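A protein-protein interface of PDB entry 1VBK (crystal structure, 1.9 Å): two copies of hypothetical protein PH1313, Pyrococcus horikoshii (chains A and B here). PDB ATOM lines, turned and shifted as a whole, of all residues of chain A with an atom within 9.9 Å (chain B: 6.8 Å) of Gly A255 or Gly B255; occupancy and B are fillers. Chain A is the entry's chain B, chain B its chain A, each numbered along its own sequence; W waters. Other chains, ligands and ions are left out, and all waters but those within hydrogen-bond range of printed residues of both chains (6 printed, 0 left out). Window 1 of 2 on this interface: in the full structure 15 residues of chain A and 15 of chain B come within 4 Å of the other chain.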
ATOM      1  N   ARG A  16       2.301 -34.258   6.126  1.00  0.00           N
ATOM      2  CA  ARG A  16       1.331 -33.551   6.951  1.00  0.00           C
ATOM      3  C   ARG A  16       1.060 -32.195   6.300  1.00  0.00           C
ATOM      4  O   ARG A  16       0.187 -31.442   6.729  1.00  0.00           O
ATOM      5  CB  ARG A  16       1.882 -33.339   8.364  1.00  0.00           C
ATOM      6  CG  ARG A  16       3.012 -32.318   8.448  1.00  0.00           C
ATOM      7  CD  ARG A  16       3.474 -32.120   9.887  1.00  0.00           C
ATOM      8  NE  ARG A  16       4.456 -31.045  10.008  1.00  0.00           N
ATOM      9  CZ  ARG A  16       5.106 -30.749  11.129  1.00  0.00           C
ATOM     10  NH1 ARG A  16       4.881 -31.450  12.233  1.00  0.00           N
ATOM     11  NH2 ARG A  16       5.976 -29.748  11.149  1.00  0.00           N
ATOM     12  N   GLY A 177      11.984 -29.433   5.843  1.00  0.00           N
ATOM     13  CA  GLY A 177      11.214 -28.302   6.317  1.00  0.00           C
ATOM     14  C   GLY A 177       9.714 -28.547   6.335  1.00  0.00           C
ATOM     15  O   GLY A 177       8.974 -27.728   6.869  1.00  0.00           O
ATOM     16  N   GLU A 179       8.297 -31.126   7.835  1.00  0.00           N
ATOM     17  CA  GLU A 179       7.961 -31.767   9.097  1.00  0.00           C
ATOM     18  C   GLU A 179       8.595 -31.094  10.315  1.00  0.00           C
ATOM     19  O   GLU A 179       8.876 -31.749  11.319  1.00  0.00           O
ATOM     20  CB  GLU A 179       8.345 -33.250   9.050  1.00  0.00           C
ATOM     21  CG  GLU A 179       7.616 -34.033   7.965  1.00  0.00           C
ATOM     22  CD  GLU A 179       6.117 -34.119   8.206  1.00  0.00           C
ATOM     23  OE1 GLU A 179       5.374 -34.439   7.250  1.00  0.00           O
ATOM     24  OE2 GLU A 179       5.685 -33.874   9.354  1.00  0.00           O
ATOM     25  N   GLY A 180       8.826 -29.787  10.221  1.00  0.00           N
ATOM     26  CA  GLY A 180       9.384 -29.055  11.347  1.00  0.00           C
ATOM     27  C   GLY A 180      10.893 -28.915  11.438  1.00  0.00           C
ATOM     28  O   GLY A 180      11.629 -29.249  10.512  1.00  0.00           O
ATOM     29  N   ARG A 181      11.346 -28.417  12.584  1.00  0.00           N
ATOM     30  CA  ARG A 181      12.764 -28.198  12.838  1.00  0.00           C
ATOM     31  C   ARG A 181      13.234 -28.837  14.145  1.00  0.00           C
ATOM     32  O   ARG A 181      12.578 -28.706  15.182  1.00  0.00           O
ATOM     33  CB  ARG A 181      13.043 -26.694  12.875  1.00  0.00           C
ATOM     34  CG  ARG A 181      14.395 -26.323  13.449  1.00  0.00           C
ATOM     35  CD  ARG A 181      14.517 -24.816  13.569  1.00  0.00           C
ATOM     36  NE  ARG A 181      14.600 -24.182  12.260  1.00  0.00           N
ATOM     37  CZ  ARG A 181      14.448 -22.879  12.048  1.00  0.00           C
ATOM     38  NH1 ARG A 181      14.189 -22.064  13.061  1.00  0.00           N
ATOM     39  NH2 ARG A 181      14.591 -22.385  10.826  1.00  0.00           N
ATOM     40  N   MET A 182      14.377 -29.517  14.088  1.00  0.00           N
ATOM     41  CA  MET A 182      14.958 -30.171  15.261  1.00  0.00           C
ATOM     42  C   MET A 182      16.464 -29.934  15.286  1.00  0.00           C
ATOM     43  O   MET A 182      17.052 -29.513  14.291  1.00  0.00           O
ATOM     44  CB  MET A 182      14.735 -31.689  15.210  1.00  0.00           C
ATOM     45  CG  MET A 182      13.289 -32.159  15.193  1.00  0.00           C
ATOM     46  SD  MET A 182      13.230 -33.960  15.302  1.00  0.00           S
ATOM     47  CE  MET A 182      11.513 -34.271  14.993  1.00  0.00           C
ATOM     48  N   ILE A 183      17.092 -30.184  16.429  1.00  0.00           N
ATOM     49  CA  ILE A 183      18.539 -30.060  16.485  1.00  0.00           C
ATOM     50  C   ILE A 183      19.042 -31.494  16.446  1.00  0.00           C
ATOM     51  O   ILE A 183      18.336 -32.419  16.849  1.00  0.00           O
ATOM     52  CB  ILE A 183      19.053 -29.377  17.780  1.00  0.00           C
ATOM     53  CG1 ILE A 183      18.566 -30.130  19.015  1.00  0.00           C
ATOM     54  CG2 ILE A 183      18.628 -27.921  17.795  1.00  0.00           C
ATOM     55  CD1 ILE A 183      19.224 -29.672  20.312  1.00  0.00           C
ATOM     56  N   VAL A 203      12.522 -33.382   8.075  1.00  0.00           N
ATOM     57  CA  VAL A 203      12.890 -32.519   9.188  1.00  0.00           C
ATOM     58  C   VAL A 203      14.113 -31.655   8.903  1.00  0.00           C
ATOM     59  O   VAL A 203      15.146 -32.149   8.446  1.00  0.00           O
ATOM     60  CB  VAL A 203      13.181 -33.350  10.459  1.00  0.00           C
ATOM     61  CG1 VAL A 203      13.542 -32.421  11.628  1.00  0.00           C
ATOM     62  CG2 VAL A 203      11.975 -34.210  10.803  1.00  0.00           C
ATOM     63  N   GLU A 204      13.980 -30.358   9.160  1.00  0.00           N
ATOM     64  CA  GLU A 204      15.080 -29.415   8.999  1.00  0.00           C
ATOM     65  C   GLU A 204      15.918 -29.571  10.271  1.00  0.00           C
ATOM     66  O   GLU A 204      15.424 -29.374  11.382  1.00  0.00           O
ATOM     67  CB  GLU A 204      14.541 -27.988   8.895  1.00  0.00           C
ATOM     68  CG  GLU A 204      15.593 -26.911   9.052  1.00  0.00           C
ATOM     69  CD  GLU A 204      14.994 -25.515   9.139  1.00  0.00           C
ATOM     70  OE1 GLU A 204      13.908 -25.363   9.741  1.00  0.00           O
ATOM     71  OE2 GLU A 204      15.618 -24.567   8.622  1.00  0.00           O
ATOM     72  N   ILE A 206      19.288 -28.658  12.681  1.00  0.00           N
ATOM     73  CA  ILE A 206      20.347 -27.738  13.065  1.00  0.00           C
ATOM     74  C   ILE A 206      21.346 -28.630  13.798  1.00  0.00           C
ATOM     75  O   ILE A 206      21.061 -29.112  14.895  1.00  0.00           O
ATOM     76  CB  ILE A 206      19.832 -26.656  14.035  1.00  0.00           C
ATOM     77  CG1 ILE A 206      18.838 -25.740  13.310  1.00  0.00           C
ATOM     78  CG2 ILE A 206      21.009 -25.860  14.600  1.00  0.00           C
ATOM     79  CD1 ILE A 206      18.150 -24.735  14.219  1.00  0.00           C
ATOM     80  N   VAL A 247      22.643 -24.937  24.537  1.00  0.00           N
ATOM     81  CA  VAL A 247      21.788 -25.826  23.762  1.00  0.00           C
ATOM     82  C   VAL A 247      20.317 -25.481  24.019  1.00  0.00           C
ATOM     83  O   VAL A 247      19.524 -25.398  23.081  1.00  0.00           O
ATOM     84  CB  VAL A 247      22.051 -27.312  24.118  1.00  0.00           C
ATOM     85  CG1 VAL A 247      21.096 -28.215  23.345  1.00  0.00           C
ATOM     86  CG2 VAL A 247      23.492 -27.680  23.785  1.00  0.00           C
ATOM     87  N   LEU A 248      19.954 -25.276  25.285  1.00  0.00           N
ATOM     88  CA  LEU A 248      18.578 -24.918  25.632  1.00  0.00           C
ATOM     89  C   LEU A 248      18.205 -23.579  24.993  1.00  0.00           C
ATOM     90  O   LEU A 248      17.085 -23.404  24.504  1.00  0.00           O
ATOM     91  CB  LEU A 248      18.405 -24.837  27.160  1.00  0.00           C
ATOM     92  CG  LEU A 248      18.486 -26.176  27.907  1.00  0.00           C
ATOM     93  CD1 LEU A 248      18.418 -25.964  29.421  1.00  0.00           C
ATOM     94  CD2 LEU A 248      17.339 -27.064  27.448  1.00  0.00           C
ATOM     95  N   LYS A 249      19.145 -22.639  24.997  1.00  0.00           N
ATOM     96  CA  LYS A 249      18.919 -21.322  24.400  1.00  0.00           C
ATOM     97  C   LYS A 249      18.671 -21.473  22.900  1.00  0.00           C
ATOM     98  O   LYS A 249      17.810 -20.797  22.332  1.00  0.00           O
ATOM     99  CB  LYS A 249      20.134 -20.416  24.633  1.00  0.00           C
ATOM    100  CG  LYS A 249      20.012 -19.012  24.044  1.00  0.00           C
ATOM    101  CD  LYS A 249      21.307 -18.227  24.253  1.00  0.00           C
ATOM    102  CE  LYS A 249      21.238 -16.815  23.682  1.00  0.00           C
ATOM    103  NZ  LYS A 249      20.320 -15.938  24.461  1.00  0.00           N
ATOM    104  N   LEU A 250      19.431 -22.361  22.265  1.00  0.00           N
ATOM    105  CA  LEU A 250      19.285 -22.612  20.834  1.00  0.00           C
ATOM    106  C   LEU A 250      17.881 -23.149  20.554  1.00  0.00           C
ATOM    107  O   LEU A 250      17.206 -22.710  19.620  1.00  0.00           O
ATOM    108  CB  LEU A 250      20.325 -23.636  20.370  1.00  0.00           C
ATOM    109  CG  LEU A 250      20.380 -23.994  18.884  1.00  0.00           C
ATOM    110  CD1 LEU A 250      20.875 -22.786  18.076  1.00  0.00           C
ATOM    111  CD2 LEU A 250      21.322 -25.179  18.690  1.00  0.00           C
ATOM    112  N   ILE A 251      17.447 -24.102  21.374  1.00  0.00           N
ATOM    113  CA  ILE A 251      16.121 -24.694  21.218  1.00  0.00           C
ATOM    114  C   ILE A 251      15.030 -23.625  21.319  1.00  0.00           C
ATOM    115  O   ILE A 251      14.092 -23.603  20.515  1.00  0.00           O
ATOM    116  CB  ILE A 251      15.879 -25.776  22.289  1.00  0.00           C
ATOM    117  CG1 ILE A 251      16.762 -26.997  21.993  1.00  0.00           C
ATOM    118  CG2 ILE A 251      14.399 -26.147  22.331  1.00  0.00           C
ATOM    119  CD1 ILE A 251      16.751 -28.046  23.085  1.00  0.00           C
ATOM    120  N   ARG A 252      15.157 -22.738  22.302  1.00  0.00           N
ATOM    121  CA  ARG A 252      14.180 -21.669  22.491  1.00  0.00           C
ATOM    122  C   ARG A 252      14.229 -20.628  21.373  1.00  0.00           C
ATOM    123  O   ARG A 252      13.204 -20.287  20.781  1.00  0.00           O
ATOM    124  CB  ARG A 252      14.408 -20.972  23.841  1.00  0.00           C
ATOM    125  CG  ARG A 252      13.693 -19.623  23.982  1.00  0.00           C
ATOM    126  CD  ARG A 252      14.169 -18.851  25.209  1.00  0.00           C
ATOM    127  NE  ARG A 252      13.596 -19.367  26.451  1.00  0.00           N
ATOM    128  CZ  ARG A 252      12.375 -19.073  26.891  1.00  0.00           C
ATOM    129  NH1 ARG A 252      11.594 -18.257  26.193  1.00  0.00           N
ATOM    130  NH2 ARG A 252      11.929 -19.605  28.022  1.00  0.00           N
ATOM    131  N   ASP A 253      15.426 -20.131  21.074  1.00  0.00           N
ATOM    132  CA  ASP A 253      15.581 -19.099  20.055  1.00  0.00           C
ATOM    133  C   ASP A 253      15.140 -19.470  18.649  1.00  0.00           C
ATOM    134  O   ASP A 253      14.678 -18.614  17.896  1.00  0.00           O
ATOM    135  CB  ASP A 253      17.032 -18.618  19.998  1.00  0.00           C
ATOM    136  CG  ASP A 253      17.443 -17.854  21.237  1.00  0.00           C
ATOM    137  OD1 ASP A 253      16.560 -17.487  22.044  1.00  0.00           O
ATOM    138  OD2 ASP A 253      18.656 -17.610  21.399  1.00  0.00           O
ATOM    139  N   PHE A 254      15.278 -20.740  18.287  1.00  0.00           N
ATOM    140  CA  PHE A 254      14.905 -21.153  16.947  1.00  0.00           C
ATOM    141  C   PHE A 254      13.638 -21.994  16.831  1.00  0.00           C
ATOM    142  O   PHE A 254      13.366 -22.562  15.775  1.00  0.00           O
ATOM    143  CB  PHE A 254      16.096 -21.857  16.296  1.00  0.00           C
ATOM    144  CG  PHE A 254      17.233 -20.925  15.987  1.00  0.00           C
ATOM    145  CD1 PHE A 254      17.224 -20.162  14.821  1.00  0.00           C
ATOM    146  CD2 PHE A 254      18.276 -20.755  16.888  1.00  0.00           C
ATOM    147  CE1 PHE A 254      18.245 -19.234  14.560  1.00  0.00           C
ATOM    148  CE2 PHE A 254      19.298 -19.834  16.641  1.00  0.00           C
ATOM    149  CZ  PHE A 254      19.277 -19.073  15.471  1.00  0.00           C
ATOM    150  N   GLY A 255      12.859 -22.056  17.908  1.00  0.00           N
ATOM    151  CA  GLY A 255      11.617 -22.815  17.881  1.00  0.00           C
ATOM    152  C   GLY A 255      11.763 -24.282  17.520  1.00  0.00           C
ATOM    153  O   GLY A 255      10.963 -24.831  16.755  1.00  0.00           O
ATOM    154  N   VAL A 256      12.792 -24.914  18.073  1.00  0.00           N
ATOM    155  CA  VAL A 256      13.081 -26.326  17.837  1.00  0.00           C
ATOM    156  C   VAL A 256      12.012 -27.181  18.516  1.00  0.00           C
ATOM    157  O   VAL A 256      11.615 -26.895  19.647  1.00  0.00           O
ATOM    158  CB  VAL A 256      14.478 -26.675  18.409  1.00  0.00           C
ATOM    159  CG1 VAL A 256      14.727 -28.171  18.345  1.00  0.00           C
ATOM    160  CG2 VAL A 256      15.550 -25.909  17.635  1.00  0.00           C
ATOM    161  N   LYS A 257      11.550 -28.232  17.840  1.00  0.00           N
ATOM    162  CA  LYS A 257      10.512 -29.079  18.424  1.00  0.00           C
ATOM    163  C   LYS A 257      10.979 -30.486  18.780  1.00  0.00           C
ATOM    164  O   LYS A 257      10.195 -31.307  19.258  1.00  0.00           O
ATOM    165  CB  LYS A 257       9.313 -29.170  17.478  1.00  0.00           C
ATOM    166  CG  LYS A 257       9.539 -30.060  16.273  1.00  0.00           C
ATOM    167  CD  LYS A 257       8.243 -30.258  15.501  1.00  0.00           C
ATOM    168  CE  LYS A 257       8.429 -31.230  14.356  1.00  0.00           C
ATOM    169  NZ  LYS A 257       7.174 -31.397  13.576  1.00  0.00           N
ATOM    170  N   GLY A 258      12.255 -30.770  18.542  1.00  0.00           N
ATOM    171  CA  GLY A 258      12.778 -32.081  18.863  1.00  0.00           C
ATOM    172  C   GLY A 258      14.292 -32.104  18.863  1.00  0.00           C
ATOM    173  O   GLY A 258      14.941 -31.165  18.392  1.00  0.00           O
ATOM    174  N   VAL A 259      14.846 -33.182  19.401  1.00  0.00           N
ATOM    175  CA  VAL A 259      16.287 -33.376  19.468  1.00  0.00           C
ATOM    176  C   VAL A 259      16.585 -34.772  18.930  1.00  0.00           C
ATOM    177  O   VAL A 259      15.930 -35.738  19.320  1.00  0.00           O
ATOM    178  CB  VAL A 259      16.794 -33.287  20.933  1.00  0.00           C
ATOM    179  CG1 VAL A 259      18.285 -33.568  20.993  1.00  0.00           C
ATOM    180  CG2 VAL A 259      16.478 -31.921  21.509  1.00  0.00           C
ATOM    181  N   PRO A 283      13.693 -30.096  26.961  1.00  0.00           N
ATOM    182  CA  PRO A 283      12.332 -29.553  27.036  1.00  0.00           C
ATOM    183  C   PRO A 283      11.430 -29.961  25.871  1.00  0.00           C
ATOM    184  O   PRO A 283      10.284 -29.524  25.782  1.00  0.00           O
ATOM    185  CB  PRO A 283      12.575 -28.051  27.068  1.00  0.00           C
ATOM    186  CG  PRO A 283      13.731 -27.905  26.133  1.00  0.00           C
ATOM    187  CD  PRO A 283      14.651 -29.041  26.574  1.00  0.00           C
ATOM    188  N   VAL A 284      11.967 -30.774  24.968  1.00  0.00           N
ATOM    189  CA  VAL A 284      11.226 -31.262  23.808  1.00  0.00           C
ATOM    190  C   VAL A 284      11.586 -32.734  23.635  1.00  0.00           C
ATOM    191  O   VAL A 284      12.584 -33.200  24.190  1.00  0.00           O
ATOM    192  CB  VAL A 284      11.595 -30.484  22.513  1.00  0.00           C
ATOM    193  CG1 VAL A 284      11.253 -29.001  22.679  1.00  0.00           C
ATOM    194  CG2 VAL A 284      13.074 -30.656  22.198  1.00  0.00           C
ATOM    195  N   ARG B 181       5.518 -21.285  20.176  1.00  0.00           N
ATOM    196  CA  ARG B 181       5.672 -19.922  19.688  1.00  0.00           C
ATOM    197  C   ARG B 181       4.858 -19.652  18.424  1.00  0.00           C
ATOM    198  O   ARG B 181       4.831 -20.466  17.502  1.00  0.00           O
ATOM    199  CB  ARG B 181       7.154 -19.647  19.417  1.00  0.00           C
ATOM    200  CG  ARG B 181       7.432 -18.443  18.535  1.00  0.00           C
ATOM    201  CD  ARG B 181       8.906 -18.374  18.192  1.00  0.00           C
ATOM    202  NE  ARG B 181       9.706 -18.029  19.362  1.00  0.00           N
ATOM    203  CZ  ARG B 181      11.022 -18.181  19.446  1.00  0.00           C
ATOM    204  NH1 ARG B 181      11.704 -18.686  18.427  1.00  0.00           N
ATOM    205  NH2 ARG B 181      11.660 -17.803  20.545  1.00  0.00           N
ATOM    206  N   MET B 182       4.207 -18.495  18.390  1.00  0.00           N
ATOM    207  CA  MET B 182       3.396 -18.096  17.243  1.00  0.00           C
ATOM    208  C   MET B 182       3.622 -16.621  16.962  1.00  0.00           C
ATOM    209  O   MET B 182       4.157 -15.901  17.802  1.00  0.00           O
ATOM    210  CB  MET B 182       1.905 -18.286  17.543  1.00  0.00           C
ATOM    211  CG  MET B 182       1.493 -19.683  17.950  1.00  0.00           C
ATOM    212  SD  MET B 182      -0.295 -19.749  18.098  1.00  0.00           S
ATOM    213  CE  MET B 182      -0.551 -21.484  18.426  1.00  0.00           C
ATOM    214  N   LYS B 249       9.311 -15.361   6.030  1.00  0.00           N
ATOM    215  CA  LYS B 249      10.702 -15.495   6.449  1.00  0.00           C
ATOM    216  C   LYS B 249      10.785 -15.579   7.971  1.00  0.00           C
ATOM    217  O   LYS B 249      11.545 -16.379   8.511  1.00  0.00           O
ATOM    218  CB  LYS B 249      11.533 -14.306   5.955  1.00  0.00           C
ATOM    219  CG  LYS B 249      13.003 -14.360   6.363  1.00  0.00           C
ATOM    220  CD  LYS B 249      13.784 -13.193   5.763  1.00  0.00           C
ATOM    221  CE  LYS B 249      15.221 -13.162   6.261  1.00  0.00           C
ATOM    222  NZ  LYS B 249      15.947 -14.422   5.944  1.00  0.00           N
ATOM    223  N   LEU B 250       9.998 -14.751   8.653  1.00  0.00           N
ATOM    224  CA  LEU B 250       9.973 -14.722  10.114  1.00  0.00           C
ATOM    225  C   LEU B 250       9.490 -16.068  10.654  1.00  0.00           C
ATOM    226  O   LEU B 250      10.055 -16.619  11.605  1.00  0.00           O
ATOM    227  CB  LEU B 250       9.034 -13.611  10.591  1.00  0.00           C
ATOM    228  CG  LEU B 250       9.103 -13.144  12.048  1.00  0.00           C
ATOM    229  CD1 LEU B 250      10.451 -12.461  12.313  1.00  0.00           C
ATOM    230  CD2 LEU B 250       7.964 -12.170  12.315  1.00  0.00           C
ATOM    231  N   ILE B 251       8.428 -16.589  10.051  1.00  0.00           N
ATOM    232  CA  ILE B 251       7.885 -17.870  10.469  1.00  0.00           C
ATOM    233  C   ILE B 251       8.951 -18.959  10.350  1.00  0.00           C
ATOM    234  O   ILE B 251       9.149 -19.750  11.278  1.00  0.00           O
ATOM    235  CB  ILE B 251       6.657 -18.244   9.618  1.00  0.00           C
ATOM    236  CG1 ILE B 251       5.496 -17.303   9.962  1.00  0.00           C
ATOM    237  CG2 ILE B 251       6.282 -19.695   9.860  1.00  0.00           C
ATOM    238  CD1 ILE B 251       4.279 -17.442   9.054  1.00  0.00           C
ATOM    239  N   ARG B 252       9.641 -18.987   9.211  1.00  0.00           N
ATOM    240  CA  ARG B 252      10.692 -19.975   8.980  1.00  0.00           C
ATOM    241  C   ARG B 252      11.887 -19.788   9.919  1.00  0.00           C
ATOM    242  O   ARG B 252      12.298 -20.727  10.606  1.00  0.00           O
ATOM    243  CB  ARG B 252      11.171 -19.913   7.522  1.00  0.00           C
ATOM    244  CG  ARG B 252      12.457 -20.703   7.253  1.00  0.00           C
ATOM    245  CD  ARG B 252      13.025 -20.423   5.861  1.00  0.00           C
ATOM    246  NE  ARG B 252      12.314 -21.131   4.795  1.00  0.00           N
ATOM    247  CZ  ARG B 252      12.437 -22.434   4.543  1.00  0.00           C
ATOM    248  NH1 ARG B 252      13.249 -23.188   5.277  1.00  0.00           N
ATOM    249  NH2 ARG B 252      11.746 -22.984   3.553  1.00  0.00           N
ATOM    250  N   ASP B 253      12.436 -18.577   9.961  1.00  0.00           N
ATOM    251  CA  ASP B 253      13.598 -18.307  10.808  1.00  0.00           C
ATOM    252  C   ASP B 253      13.417 -18.571  12.301  1.00  0.00           C
ATOM    253  O   ASP B 253      14.334 -19.060  12.962  1.00  0.00           O
ATOM    254  CB  ASP B 253      14.070 -16.862  10.617  1.00  0.00           C
ATOM    255  CG  ASP B 253      14.653 -16.615   9.243  1.00  0.00           C
ATOM    256  OD1 ASP B 253      14.931 -17.595   8.521  1.00  0.00           O
ATOM    257  OD2 ASP B 253      14.843 -15.432   8.888  1.00  0.00           O
ATOM    258  N   PHE B 254      12.245 -18.261  12.840  1.00  0.00           N
ATOM    259  CA  PHE B 254      12.014 -18.456  14.267  1.00  0.00           C
ATOM    260  C   PHE B 254      11.290 -19.738  14.673  1.00  0.00           C
ATOM    261  O   PHE B 254      11.025 -19.955  15.853  1.00  0.00           O
ATOM    262  CB  PHE B 254      11.286 -17.233  14.826  1.00  0.00           C
ATOM    263  CG  PHE B 254      12.156 -16.010  14.900  1.00  0.00           C
ATOM    264  CD1 PHE B 254      12.959 -15.780  16.012  1.00  0.00           C
ATOM    265  CD2 PHE B 254      12.223 -15.123  13.831  1.00  0.00           C
ATOM    266  CE1 PHE B 254      13.820 -14.684  16.061  1.00  0.00           C
ATOM    267  CE2 PHE B 254      13.080 -14.024  13.867  1.00  0.00           C
ATOM    268  CZ  PHE B 254      13.880 -13.804  14.983  1.00  0.00           C
ATOM    269  N   GLY B 255      10.975 -20.587  13.703  1.00  0.00           N
ATOM    270  CA  GLY B 255      10.293 -21.832  14.017  1.00  0.00           C
ATOM    271  C   GLY B 255       8.907 -21.635  14.602  1.00  0.00           C
ATOM    272  O   GLY B 255       8.506 -22.342  15.522  1.00  0.00           O
ATOM    273  N   VAL B 256       8.176 -20.667  14.061  1.00  0.00           N
ATOM    274  CA  VAL B 256       6.817 -20.348  14.496  1.00  0.00           C
ATOM    275  C   VAL B 256       5.877 -21.503  14.137  1.00  0.00           C
ATOM    276  O   VAL B 256       5.916 -22.014  13.018  1.00  0.00           O
ATOM    277  CB  VAL B 256       6.337 -19.047  13.801  1.00  0.00           C
ATOM    278  CG1 VAL B 256       4.862 -18.819  14.048  1.00  0.00           C
ATOM    279  CG2 VAL B 256       7.161 -17.863  14.310  1.00  0.00           C
ATOM    280  N   LYS B 257       5.029 -21.900  15.083  1.00  0.00           N
ATOM    281  CA  LYS B 257       4.099 -23.008  14.871  1.00  0.00           C
ATOM    282  C   LYS B 257       2.671 -22.567  14.566  1.00  0.00           C
ATOM    283  O   LYS B 257       1.813 -23.394  14.251  1.00  0.00           O
ATOM    284  CB  LYS B 257       4.085 -23.917  16.106  1.00  0.00           C
ATOM    285  CG  LYS B 257       3.553 -23.229  17.355  1.00  0.00           C
ATOM    286  CD  LYS B 257       3.650 -24.115  18.591  1.00  0.00           C
ATOM    287  CE  LYS B 257       2.697 -25.293  18.519  1.00  0.00           C
ATOM    288  NZ  LYS B 257       2.792 -26.118  19.754  1.00  0.00           N
ATOM    289  N   GLY B 258       2.412 -21.269  14.659  1.00  0.00           N
ATOM    290  CA  GLY B 258       1.071 -20.785  14.396  1.00  0.00           C
ATOM    291  C   GLY B 258       0.986 -19.286  14.200  1.00  0.00           C
ATOM    292  O   GLY B 258       1.922 -18.550  14.505  1.00  0.00           O
HETATM  293  O   HOH W   1      14.169 -15.821  19.376  1.00  0.00           O
HETATM  294  O   HOH W   2       7.998 -24.871  16.675  1.00  0.00           O
HETATM  295  O   HOH W   3      13.920 -16.605  21.959  1.00  0.00           O
HETATM  296  O   HOH W   4      15.617 -22.636   7.069  1.00  0.00           O
HETATM  297  O   HOH W   5      10.759 -21.001  21.409  1.00  0.00           O
HETATM  298  O   HOH W   6      15.801 -20.292   8.885  1.00  0.00           O
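Among the printed residues, 12 pairs touch across the chains.
NZ of Lys B249 is in salt-bridge range of OD2 of Asp B253, at 3.3 Å. NZ of Lys A249 is in salt-bridge range of OD2 of Asp A253. The backbone carbonyl oxygen (O) of Arg B181 lies within hydrogen-bond range of the backbone NH (N) of Lys B257. The guanidinium group of Arg B181 lies within hydrogen-bond range of the backbone carbonyl oxygen of Phe B254. NH1 of Arg A181 sits at hydrogen-bond distance from O of Phe A254, at 2.9 Å. N of Lys A257 is in hydrogen-bond range of O of Arg A181.
Of chain B, only Arg B181 (3.6 Å), Phe B254 (3.5 Å) and Gly B255 (3.7 Å) come within 4 Å of Gly A255. Gly B255 touches just these residues of chain A: Arg A181, Phe A254 and Gly A255. Of chain A, only Arg A252, Asp A253 and Gly A255 come within 4 Å of Arg B181. No residue of chain A comes within 4 Å of Val B256. Printed residues of chain B within 4 Å of Arg A181: Arg B252, Asp B253 and Gly B255. Printed residues of chain A within 4 Å of Phe B254: Asp A253 (3.8 Å), Phe A254 (3.5 Å) and Gly A255 (3.5 Å). Printed residues of chain B within 4 Å of Arg A252: Arg B181. Pro A283 touches none of the printed residues of chain B. The nearest printed residue of chain B that does not touch Arg A252 is Phe B254 (5.4 Å).
NH2 of Arg B181 sits at hydrogen-bond distance from O of Arg A252 (2.9 Å). O of Phe B254 lies within hydrogen-bond range of N of Gly A255, at 3.5 Å. The backbone carbonyl oxygen of Asp A253 lies within hydrogen-bond range of the guanidinium group of Arg B181 (3.0 Å). The backbone carbonyl oxygen (O) of Arg B252 is in hydrogen-bond range of the guanidinium group (NH2) of Arg A181, at 2.8 Å. The backbone carbonyl oxygen (O) of Asp B253 sits at hydrogen-bond distance from the guanidinium group (NH1) of Arg A181 (3.0 Å).
Gly B255 touches Arg A181. Asp A253 touches Phe B254. CD1 of Phe A254 touches O of Asp B253 (3.6 Å). Phe A254 touches Phe B254. Phe A254 touches Gly B255. Gly A255 touches Arg B181. Gly A255 touches Gly B255.
Arg A181 touches Arg B252, and with the chains exchanged Arg A252 touches Arg B181. Arg A181 touches Gly B255, and with the chains exchanged Gly A255 touches Arg B181. Phe A254 touches Gly B255, and with the chains exchanged Gly A255 touches Phe B254. Gly B255 touches its own counterpart, Gly A255. 12 positions are printed for both chains.
Water W4 lies within hydrogen-bond range of the side-chain carboxylate (OE2) of Glu A204 (2.5 Å) and the guanidinium group (NH1) of Arg B252 (3.0 Å). Water W5 lies within hydrogen-bond range of O of Arg A252 (2.6 Å) and NH2 of Arg B181 (3.4 Å). Water W3 bridges the side-chain carboxylate (OD1) of Asp A253 (2.8 Å) and the guanidinium group (NH2) of Arg B181 (2.9 Å). Water W2 lies within hydrogen-bond range of the backbone carbonyl oxygen of Gly B255 (2.8 Å) and the backbone carbonyl oxygen of Gly A255 (3.0 Å). Water W6 lies within hydrogen-bond range of the side-chain carboxylate (OD1) of Asp B253 and the guanidinium group (NH2) of Arg A181. Water W1 bridges O of Asp A253 (3.2 Å) and NH2 of Arg B181 (3.4 Å).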
